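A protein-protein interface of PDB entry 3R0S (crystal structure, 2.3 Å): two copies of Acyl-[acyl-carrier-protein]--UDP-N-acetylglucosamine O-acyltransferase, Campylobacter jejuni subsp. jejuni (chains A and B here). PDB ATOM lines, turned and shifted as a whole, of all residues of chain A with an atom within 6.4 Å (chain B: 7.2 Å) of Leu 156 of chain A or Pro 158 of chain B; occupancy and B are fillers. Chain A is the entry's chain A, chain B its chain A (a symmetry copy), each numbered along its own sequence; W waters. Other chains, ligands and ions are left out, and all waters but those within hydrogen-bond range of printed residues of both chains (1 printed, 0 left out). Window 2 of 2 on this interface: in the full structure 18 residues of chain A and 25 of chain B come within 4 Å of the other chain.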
ATOM      1  N   ALA A 136      15.910  10.180 -13.182  1.00  0.00           N
ATOM      2  CA  ALA A 136      15.651  10.696 -14.506  1.00  0.00           C
ATOM      3  C   ALA A 136      14.384  11.541 -14.467  1.00  0.00           C
ATOM      4  O   ALA A 136      13.688  11.586 -13.431  1.00  0.00           O
ATOM      5  CB  ALA A 136      15.522   9.525 -15.519  1.00  0.00           C
ATOM      6  N   ASN A 137      14.053  12.176 -15.585  1.00  0.00           N
ATOM      7  CA  ASN A 137      12.966  13.166 -15.616  1.00  0.00           C
ATOM      8  C   ASN A 137      11.644  12.630 -15.070  1.00  0.00           C
ATOM      9  O   ASN A 137      11.249  11.505 -15.404  1.00  0.00           O
ATOM     10  CB  ASN A 137      12.720  13.679 -17.026  1.00  0.00           C
ATOM     11  CG  ASN A 137      13.976  14.236 -17.668  1.00  0.00           C
ATOM     12  OD1 ASN A 137      14.433  15.276 -17.315  1.00  0.00           O
ATOM     13  ND2 ASN A 137      14.548  13.488 -18.592  1.00  0.00           N
ATOM     14  N   ASN A 138      11.016  13.431 -14.202  1.00  0.00           N
ATOM     15  CA  ASN A 138       9.764  13.145 -13.579  1.00  0.00           C
ATOM     16  C   ASN A 138       9.701  11.902 -12.647  1.00  0.00           C
ATOM     17  O   ASN A 138       8.656  11.525 -12.271  1.00  0.00           O
ATOM     18  CB  ASN A 138       8.687  12.981 -14.617  1.00  0.00           C
ATOM     19  CG  ASN A 138       8.594  14.149 -15.596  1.00  0.00           C
ATOM     20  OD1 ASN A 138       9.078  14.025 -16.716  1.00  0.00           O
ATOM     21  ND2 ASN A 138       7.877  15.250 -15.211  1.00  0.00           N
ATOM     22  N   ALA A 139      10.791  11.270 -12.302  1.00  0.00           N
ATOM     23  CA  ALA A 139      10.737  10.256 -11.292  1.00  0.00           C
ATOM     24  C   ALA A 139      10.178  10.932 -10.028  1.00  0.00           C
ATOM     25  O   ALA A 139      10.555  12.086  -9.696  1.00  0.00           O
ATOM     26  CB  ALA A 139      12.154   9.652 -11.017  1.00  0.00           C
ATOM     27  N   THR A 140       9.274  10.208  -9.355  1.00  0.00           N
ATOM     28  CA  THR A 140       8.603  10.703  -8.175  1.00  0.00           C
ATOM     29  C   THR A 140       8.685   9.723  -6.999  1.00  0.00           C
ATOM     30  O   THR A 140       8.214   8.607  -7.064  1.00  0.00           O
ATOM     31  CB  THR A 140       7.162  10.934  -8.570  1.00  0.00           C
ATOM     32  OG1 THR A 140       7.181  11.764  -9.734  1.00  0.00           O
ATOM     33  CG2 THR A 140       6.367  11.590  -7.478  1.00  0.00           C
ATOM     34  N   GLY A 154      14.419   5.364 -13.427  1.00  0.00           N
ATOM     35  CA  GLY A 154      14.144   5.932 -14.711  1.00  0.00           C
ATOM     36  C   GLY A 154      12.940   6.857 -14.733  1.00  0.00           C
ATOM     37  O   GLY A 154      12.242   7.090 -13.733  1.00  0.00           O
ATOM     38  N   GLY A 155      12.694   7.368 -15.922  1.00  0.00           N
ATOM     39  CA  GLY A 155      11.855   8.532 -16.074  1.00  0.00           C
ATOM     40  C   GLY A 155      10.393   8.212 -16.025  1.00  0.00           C
ATOM     41  O   GLY A 155       9.986   7.201 -16.535  1.00  0.00           O
ATOM     42  N   LEU A 156       9.615   9.131 -15.455  1.00  0.00           N
ATOM     43  CA  LEU A 156       8.153   9.003 -15.329  1.00  0.00           C
ATOM     44  C   LEU A 156       7.729   7.808 -14.436  1.00  0.00           C
ATOM     45  O   LEU A 156       6.658   7.264 -14.634  1.00  0.00           O
ATOM     46  CB  LEU A 156       7.503   8.906 -16.706  1.00  0.00           C
ATOM     47  CG  LEU A 156       7.679  10.162 -17.559  1.00  0.00           C
ATOM     48  CD1 LEU A 156       7.470   9.866 -19.029  1.00  0.00           C
ATOM     49  CD2 LEU A 156       6.727  11.282 -17.102  1.00  0.00           C
ATOM     50  N   THR A 157       8.600   7.390 -13.517  1.00  0.00           N
ATOM     51  CA  THR A 157       8.308   6.338 -12.549  1.00  0.00           C
ATOM     52  C   THR A 157       8.101   6.844 -11.108  1.00  0.00           C
ATOM     53  O   THR A 157       8.979   7.482 -10.551  1.00  0.00           O
ATOM     54  CB  THR A 157       9.412   5.278 -12.549  1.00  0.00           C
ATOM     55  OG1 THR A 157       9.401   4.631 -13.819  1.00  0.00           O
ATOM     56  CG2 THR A 157       9.155   4.222 -11.438  1.00  0.00           C
ATOM     57  N   PRO A 158       6.909   6.591 -10.535  1.00  0.00           N
ATOM     58  CA  PRO A 158       6.572   6.827  -9.164  1.00  0.00           C
ATOM     59  C   PRO A 158       6.835   5.602  -8.297  1.00  0.00           C
ATOM     60  O   PRO A 158       6.583   4.450  -8.695  1.00  0.00           O
ATOM     61  CB  PRO A 158       5.059   7.131  -9.205  1.00  0.00           C
ATOM     62  CG  PRO A 158       4.543   6.399 -10.358  1.00  0.00           C
ATOM     63  CD  PRO A 158       5.735   6.146 -11.301  1.00  0.00           C
ATOM     64  N   ALA A 172      13.278   0.798 -13.670  1.00  0.00           N
ATOM     65  CA  ALA A 172      13.128   1.226 -15.030  1.00  0.00           C
ATOM     66  C   ALA A 172      12.104   2.365 -15.174  1.00  0.00           C
ATOM     67  O   ALA A 172      11.281   2.619 -14.289  1.00  0.00           O
ATOM     68  CB  ALA A 172      12.713   0.020 -15.914  1.00  0.00           C
ATOM     69  N   GLY A 173      12.171   3.050 -16.302  1.00  0.00           N
ATOM     70  CA  GLY A 173      11.333   4.200 -16.533  1.00  0.00           C
ATOM     71  C   GLY A 173       9.983   3.632 -16.956  1.00  0.00           C
ATOM     72  O   GLY A 173       9.880   2.435 -17.309  1.00  0.00           O
ATOM     73  N   ALA A 174       8.967   4.488 -16.844  1.00  0.00           N
ATOM     74  CA  ALA A 174       7.610   4.232 -17.318  1.00  0.00           C
ATOM     75  C   ALA A 174       7.097   2.992 -16.645  1.00  0.00           C
ATOM     76  O   ALA A 174       6.496   2.162 -17.253  1.00  0.00           O
ATOM     77  CB  ALA A 174       7.562   4.133 -18.826  1.00  0.00           C
ATOM     78  N   SER A 175       7.416   2.899 -15.372  1.00  0.00           N
ATOM     79  CA  SER A 175       6.963   1.860 -14.473  1.00  0.00           C
ATOM     80  C   SER A 175       6.318   2.463 -13.193  1.00  0.00           C
ATOM     81  O   SER A 175       6.235   3.678 -13.066  1.00  0.00           O
ATOM     82  CB  SER A 175       8.209   1.011 -14.141  1.00  0.00           C
ATOM     83  OG  SER A 175       8.737   0.475 -15.356  1.00  0.00           O
ATOM     84  N   ALA A 176       5.839   1.626 -12.267  1.00  0.00           N
ATOM     85  CA  ALA A 176       5.260   2.092 -10.977  1.00  0.00           C
ATOM     86  C   ALA A 176       5.528   1.088  -9.846  1.00  0.00           C
ATOM     87  O   ALA A 176       5.052  -0.049  -9.906  1.00  0.00           O
ATOM     88  CB  ALA A 176       3.757   2.338 -11.114  1.00  0.00           C
ATOM     89  N   ASN B 138       4.236  16.879 -20.908  1.00  0.00           N
ATOM     90  CA  ASN B 138       5.220  15.967 -20.419  1.00  0.00           C
ATOM     91  C   ASN B 138       5.821  14.955 -21.435  1.00  0.00           C
ATOM     92  O   ASN B 138       6.483  14.073 -21.036  1.00  0.00           O
ATOM     93  CB  ASN B 138       4.669  15.172 -19.267  1.00  0.00           C
ATOM     94  CG  ASN B 138       4.072  16.031 -18.155  1.00  0.00           C
ATOM     95  OD1 ASN B 138       2.853  16.146 -18.084  1.00  0.00           O
ATOM     96  ND2 ASN B 138       4.926  16.553 -17.221  1.00  0.00           N
ATOM     97  N   ALA B 139       5.576  15.067 -22.713  1.00  0.00           N
ATOM     98  CA  ALA B 139       6.291  14.253 -23.649  1.00  0.00           C
ATOM     99  C   ALA B 139       7.784  14.558 -23.439  1.00  0.00           C
ATOM    100  O   ALA B 139       8.179  15.738 -23.250  1.00  0.00           O
ATOM    101  CB  ALA B 139       5.864  14.570 -25.121  1.00  0.00           C
ATOM    102  N   THR B 140       8.587  13.485 -23.455  1.00  0.00           N
ATOM    103  CA  THR B 140      10.009  13.574 -23.221  1.00  0.00           C
ATOM    104  C   THR B 140      10.828  12.873 -24.311  1.00  0.00           C
ATOM    105  O   THR B 140      10.717  11.684 -24.527  1.00  0.00           O
ATOM    106  CB  THR B 140      10.260  12.930 -21.876  1.00  0.00           C
ATOM    107  OG1 THR B 140       9.382  13.565 -20.943  1.00  0.00           O
ATOM    108  CG2 THR B 140      11.685  13.077 -21.429  1.00  0.00           C
ATOM    109  N   LEU B 141      11.657  13.625 -24.989  1.00  0.00           N
ATOM    110  CA  LEU B 141      12.609  13.093 -25.953  1.00  0.00           C
ATOM    111  C   LEU B 141      14.008  12.996 -25.352  1.00  0.00           C
ATOM    112  O   LEU B 141      14.579  14.002 -24.914  1.00  0.00           O
ATOM    113  CB  LEU B 141      12.619  14.016 -27.141  1.00  0.00           C
ATOM    114  CG  LEU B 141      11.269  14.498 -27.670  1.00  0.00           C
ATOM    115  CD1 LEU B 141      11.501  15.213 -29.035  1.00  0.00           C
ATOM    116  CD2 LEU B 141      10.265  13.393 -27.803  1.00  0.00           C
ATOM    117  N   ALA B 142      14.555  11.787 -25.285  1.00  0.00           N
ATOM    118  CA  ALA B 142      15.903  11.562 -24.840  1.00  0.00           C
ATOM    119  C   ALA B 142      16.887  12.011 -25.928  1.00  0.00           C
ATOM    120  O   ALA B 142      16.482  12.602 -26.888  1.00  0.00           O
ATOM    121  CB  ALA B 142      16.108  10.136 -24.448  1.00  0.00           C
ATOM    122  N   VAL B 153       3.418  13.651 -30.598  1.00  0.00           N
ATOM    123  CA  VAL B 153       3.714  12.769 -29.488  1.00  0.00           C
ATOM    124  C   VAL B 153       2.786  13.114 -28.345  1.00  0.00           C
ATOM    125  O   VAL B 153       2.833  14.195 -27.800  1.00  0.00           O
ATOM    126  CB  VAL B 153       5.191  12.927 -29.021  1.00  0.00           C
ATOM    127  CG1 VAL B 153       5.450  12.008 -27.892  1.00  0.00           C
ATOM    128  CG2 VAL B 153       6.217  12.694 -30.202  1.00  0.00           C
ATOM    129  N   GLY B 154       1.923  12.197 -27.978  1.00  0.00           N
ATOM    130  CA  GLY B 154       0.995  12.443 -26.917  1.00  0.00           C
ATOM    131  C   GLY B 154       1.636  12.524 -25.543  1.00  0.00           C
ATOM    132  O   GLY B 154       2.853  12.373 -25.349  1.00  0.00           O
ATOM    133  N   GLY B 155       0.770  12.745 -24.575  1.00  0.00           N
ATOM    134  CA  GLY B 155       1.203  13.223 -23.284  1.00  0.00           C
ATOM    135  C   GLY B 155       1.745  12.135 -22.408  1.00  0.00           C
ATOM    136  O   GLY B 155       1.232  11.047 -22.421  1.00  0.00           O
ATOM    137  N   LEU B 156       2.750  12.482 -21.605  1.00  0.00           N
ATOM    138  CA  LEU B 156       3.401  11.557 -20.661  1.00  0.00           C
ATOM    139  C   LEU B 156       4.116  10.379 -21.373  1.00  0.00           C
ATOM    140  O   LEU B 156       4.239   9.316 -20.793  1.00  0.00           O
ATOM    141  CB  LEU B 156       2.396  11.040 -19.638  1.00  0.00           C
ATOM    142  CG  LEU B 156       1.826  12.131 -18.731  1.00  0.00           C
ATOM    143  CD1 LEU B 156       0.523  11.695 -18.092  1.00  0.00           C
ATOM    144  CD2 LEU B 156       2.839  12.539 -17.647  1.00  0.00           C
ATOM    145  N   THR B 157       4.517  10.573 -22.630  1.00  0.00           N
ATOM    146  CA  THR B 157       5.278   9.591 -23.394  1.00  0.00           C
ATOM    147  C   THR B 157       6.759   9.964 -23.607  1.00  0.00           C
ATOM    148  O   THR B 157       7.053  11.013 -24.153  1.00  0.00           O
ATOM    149  CB  THR B 157       4.630   9.341 -24.757  1.00  0.00           C
ATOM    150  OG1 THR B 157       3.357   8.738 -24.535  1.00  0.00           O
ATOM    151  CG2 THR B 157       5.504   8.383 -25.612  1.00  0.00           C
ATOM    152  N   PRO B 158       7.681   9.111 -23.121  1.00  0.00           N
ATOM    153  CA  PRO B 158       9.092   9.184 -23.349  1.00  0.00           C
ATOM    154  C   PRO B 158       9.512   8.368 -24.567  1.00  0.00           C
ATOM    155  O   PRO B 158       9.010   7.256 -24.816  1.00  0.00           O
ATOM    156  CB  PRO B 158       9.704   8.578 -22.069  1.00  0.00           C
ATOM    157  CG  PRO B 158       8.714   7.625 -21.574  1.00  0.00           C
ATOM    158  CD  PRO B 158       7.354   8.042 -22.165  1.00  0.00           C
ATOM    159  N   ILE B 159      10.421   8.957 -25.313  1.00  0.00           N
ATOM    160  CA  ILE B 159      11.060   8.349 -26.446  1.00  0.00           C
ATOM    161  C   ILE B 159      12.551   8.134 -26.131  1.00  0.00           C
ATOM    162  O   ILE B 159      13.259   9.078 -25.732  1.00  0.00           O
ATOM    163  CB  ILE B 159      10.885   9.221 -27.652  1.00  0.00           C
ATOM    164  CG1 ILE B 159       9.398   9.448 -27.900  1.00  0.00           C
ATOM    165  CG2 ILE B 159      11.604   8.599 -28.904  1.00  0.00           C
ATOM    166  CD1 ILE B 159       9.101  10.252 -29.121  1.00  0.00           C
ATOM    167  N   HIS B 160      12.989   6.878 -26.300  1.00  0.00           N
ATOM    168  CA  HIS B 160      14.347   6.433 -26.054  1.00  0.00           C
ATOM    169  C   HIS B 160      15.381   7.147 -26.940  1.00  0.00           C
ATOM    170  O   HIS B 160      15.098   7.556 -28.081  1.00  0.00           O
ATOM    171  CB  HIS B 160      14.397   4.926 -26.256  1.00  0.00           C
ATOM    172  CG  HIS B 160      15.717   4.291 -25.946  1.00  0.00           C
ATOM    173  ND1 HIS B 160      16.835   4.478 -26.736  1.00  0.00           N
ATOM    174  CD2 HIS B 160      16.076   3.404 -24.984  1.00  0.00           C
ATOM    175  CE1 HIS B 160      17.834   3.748 -26.254  1.00  0.00           C
ATOM    176  NE2 HIS B 160      17.404   3.105 -25.180  1.00  0.00           N
ATOM    177  N   ILE B 171       2.588   9.202 -32.126  1.00  0.00           N
ATOM    178  CA  ILE B 171       2.966   8.413 -30.963  1.00  0.00           C
ATOM    179  C   ILE B 171       2.021   8.735 -29.812  1.00  0.00           C
ATOM    180  O   ILE B 171       2.072   9.822 -29.253  1.00  0.00           O
ATOM    181  CB  ILE B 171       4.431   8.692 -30.524  1.00  0.00           C
ATOM    182  CG1 ILE B 171       5.400   8.701 -31.734  1.00  0.00           C
ATOM    183  CG2 ILE B 171       4.834   7.749 -29.367  1.00  0.00           C
ATOM    184  CD1 ILE B 171       5.494   7.381 -32.555  1.00  0.00           C
ATOM    185  N   ALA B 172       1.188   7.779 -29.446  1.00  0.00           N
ATOM    186  CA  ALA B 172       0.114   7.978 -28.517  1.00  0.00           C
ATOM    187  C   ALA B 172       0.620   8.330 -27.108  1.00  0.00           C
ATOM    188  O   ALA B 172       1.786   8.119 -26.760  1.00  0.00           O
ATOM    189  CB  ALA B 172      -0.773   6.705 -28.463  1.00  0.00           C
ATOM    190  N   ALA B 174       0.779   8.221 -22.973  1.00  0.00           N
ATOM    191  CA  ALA B 174       0.824   7.220 -21.910  1.00  0.00           C
ATOM    192  C   ALA B 174       1.366   5.944 -22.484  1.00  0.00           C
ATOM    193  O   ALA B 174       0.878   4.889 -22.218  1.00  0.00           O
ATOM    194  CB  ALA B 174      -0.533   7.036 -21.269  1.00  0.00           C
ATOM    195  N   SER B 175       2.366   6.111 -23.322  1.00  0.00           N
ATOM    196  CA  SER B 175       3.131   5.046 -23.932  1.00  0.00           C
ATOM    197  C   SER B 175       4.656   5.242 -23.703  1.00  0.00           C
ATOM    198  O   SER B 175       5.057   6.203 -23.058  1.00  0.00           O
ATOM    199  CB  SER B 175       2.769   5.067 -25.432  1.00  0.00           C
ATOM    200  OG  SER B 175       1.361   4.862 -25.570  1.00  0.00           O
ATOM    201  N   ALA B 176       5.497   4.329 -24.199  1.00  0.00           N
ATOM    202  CA  ALA B 176       6.977   4.452 -24.096  1.00  0.00           C
ATOM    203  C   ALA B 176       7.679   3.833 -25.315  1.00  0.00           C
ATOM    204  O   ALA B 176       7.569   2.625 -25.540  1.00  0.00           O
ATOM    205  CB  ALA B 176       7.487   3.797 -22.811  1.00  0.00           C
ATOM    206  N   LEU B 177       8.427   4.655 -26.042  1.00  0.00           N
ATOM    207  CA  LEU B 177       8.956   4.321 -27.368  1.00  0.00           C
ATOM    208  C   LEU B 177      10.479   4.091 -27.370  1.00  0.00           C
ATOM    209  O   LEU B 177      11.256   4.989 -26.994  1.00  0.00           O
ATOM    210  CB  LEU B 177       8.638   5.431 -28.392  1.00  0.00           C
ATOM    211  CG  LEU B 177       9.049   5.127 -29.832  1.00  0.00           C
ATOM    212  CD1 LEU B 177       8.286   3.906 -30.379  1.00  0.00           C
ATOM    213  CD2 LEU B 177       8.865   6.355 -30.760  1.00  0.00           C
ATOM    214  N   SER B 178      10.844   2.883 -27.805  1.00  0.00           N
ATOM    215  CA  SER B 178      12.227   2.410 -27.912  1.00  0.00           C
ATOM    216  C   SER B 178      12.762   2.202 -29.329  1.00  0.00           C
ATOM    217  O   SER B 178      13.973   2.123 -29.487  1.00  0.00           O
ATOM    218  CB  SER B 178      12.354   1.068 -27.216  1.00  0.00           C
ATOM    219  OG  SER B 178      12.326   1.314 -25.840  1.00  0.00           O
ATOM    220  N   GLY B 189       1.736   1.901 -26.859  1.00  0.00           N
ATOM    221  CA  GLY B 189       2.084   0.858 -25.913  1.00  0.00           C
ATOM    222  C   GLY B 189       3.394   1.142 -25.191  1.00  0.00           C
ATOM    223  O   GLY B 189       4.007   2.222 -25.316  1.00  0.00           O
ATOM    224  N   ARG B 191       6.544  -1.641 -24.368  1.00  0.00           N
ATOM    225  CA  ARG B 191       7.153  -0.807 -25.413  1.00  0.00           C
ATOM    226  C   ARG B 191       6.180  -0.597 -26.564  1.00  0.00           C
ATOM    227  O   ARG B 191       5.396  -1.510 -26.937  1.00  0.00           O
ATOM    228  CB  ARG B 191       8.454  -1.429 -25.946  1.00  0.00           C
ATOM    229  CG  ARG B 191       9.573  -1.588 -24.898  1.00  0.00           C
ATOM    230  CD  ARG B 191      10.141  -0.238 -24.501  1.00  0.00           C
ATOM    231  NE  ARG B 191      11.259  -0.337 -23.552  1.00  0.00           N
ATOM    232  CZ  ARG B 191      11.258   0.139 -22.300  1.00  0.00           C
ATOM    233  NH1 ARG B 191      10.186   0.751 -21.781  1.00  0.00           N
ATOM    234  NH2 ARG B 191      12.352   0.007 -21.552  1.00  0.00           N
ATOM    235  N   ALA B 192       6.229   0.607 -27.110  1.00  0.00           N
ATOM    236  CA  ALA B 192       5.267   1.035 -28.077  1.00  0.00           C
ATOM    237  C   ALA B 192       5.548   0.432 -29.433  1.00  0.00           C
ATOM    238  O   ALA B 192       6.710   0.274 -29.855  1.00  0.00           O
ATOM    239  CB  ALA B 192       5.247   2.556 -28.153  1.00  0.00           C
HETATM  240  O   HOH W   1       7.833  16.408 -18.088  1.00  0.00           O
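The backbone NH of Ala 176 of chain B sits at hydrogen-bond distance from the backbone carbonyl oxygen of Gly 189 of chain B.
The side-chain hydroxyl of Thr 140 of chain A is in hydrogen-bond range of the backbone carbonyl oxygen of Asn 138 of chain A.
N of Leu 177 of chain B lies within hydrogen-bond range of O of Pro 158 of chain B (2.9 Å).
N of Ala 174 of chain A is in hydrogen-bond range of O of Gly 155 of chain A, 2.9 Å away.
The side-chain hydroxyl (OG1) of Thr 157 of chain A sits at hydrogen-bond distance from the backbone NH (N) of Ala 174 of chain A (3.1 Å).
O of Ala 176 of chain B is in hydrogen-bond range of N of Ala 192 of chain B.
Among the printed residues, merely in contact across the chains: Asn 138 of chain A with Asn 138 of chain B (3.8 Å), Leu 156 of chain A with Leu 156 of chain B (3.7 Å), Leu 156 of chain A with Pro 158 of chain B (3.6 Å) and Ala 174 of chain A with Ala 176 of chain B (3.9998 Å).
Of chain B, only Leu 156 (3.7 Å) and Pro 158 (3.6 Å) come within 4 Å of Leu 156 of chain A.
Printed residues of chain B within 4 Å of Ala 174 of chain A: Ala 176 (3.9998 Å).
Printed residues of chain A within 4 Å of Asn 138 of chain B: Asn 138 (3.8 Å).
Pro 158 of chain B touches one residue of chain A.
Printed residues of chain A within 4 Å of Ala 176 of chain B: Ala 174.
The nearest residue of chain A that does not touch Pro 158 of chain B is Ala 174 of chain A (4.6 Å).
The nearest printed residue of chain B that does not touch Ala 174 of chain A is Pro 158 of chain B (4.6 Å).
Hydrophobic or aromatic side chains of chain A that line the printed part of chain B: Leu 156 and Ala 174.
Along chain B the printed residues that touch a printed residue of chain A span positions 138 to 176.
Among the printed residues, 4 pairs touch across the chains.
Among the printed residues, no Asp or Glu carboxylate lies within 4 Å of a Lys or Arg side-chain nitrogen of the other chain.
Asn 138 of chain A touches its own counterpart, Asn 138 of chain B.
Leu 156 of chain B touches its own counterpart, Leu 156 of chain A.
Leu 156 of chain A touches Pro 158 of chain B, but with the chains exchanged Pro 158 of chain A does not touch Leu 156 of chain B (9.5 Å).
Ala 174 of chain A touches Ala 176 of chain B, but with the chains exchanged Ala 176 of chain A does not touch Ala 174 of chain B (11.6 Å).
Of the 4 pairs that touch across the chains among the printed residues, 2 have their exchanged pair printed and touching as well.
Water W1 lies within hydrogen-bond range of the side-chain amide oxygen (OD1) of Asn 138 of chain A (3.0 Å) and the side-chain amide nitrogen (ND2) of Asn 138 of chain B (3.0 Å).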
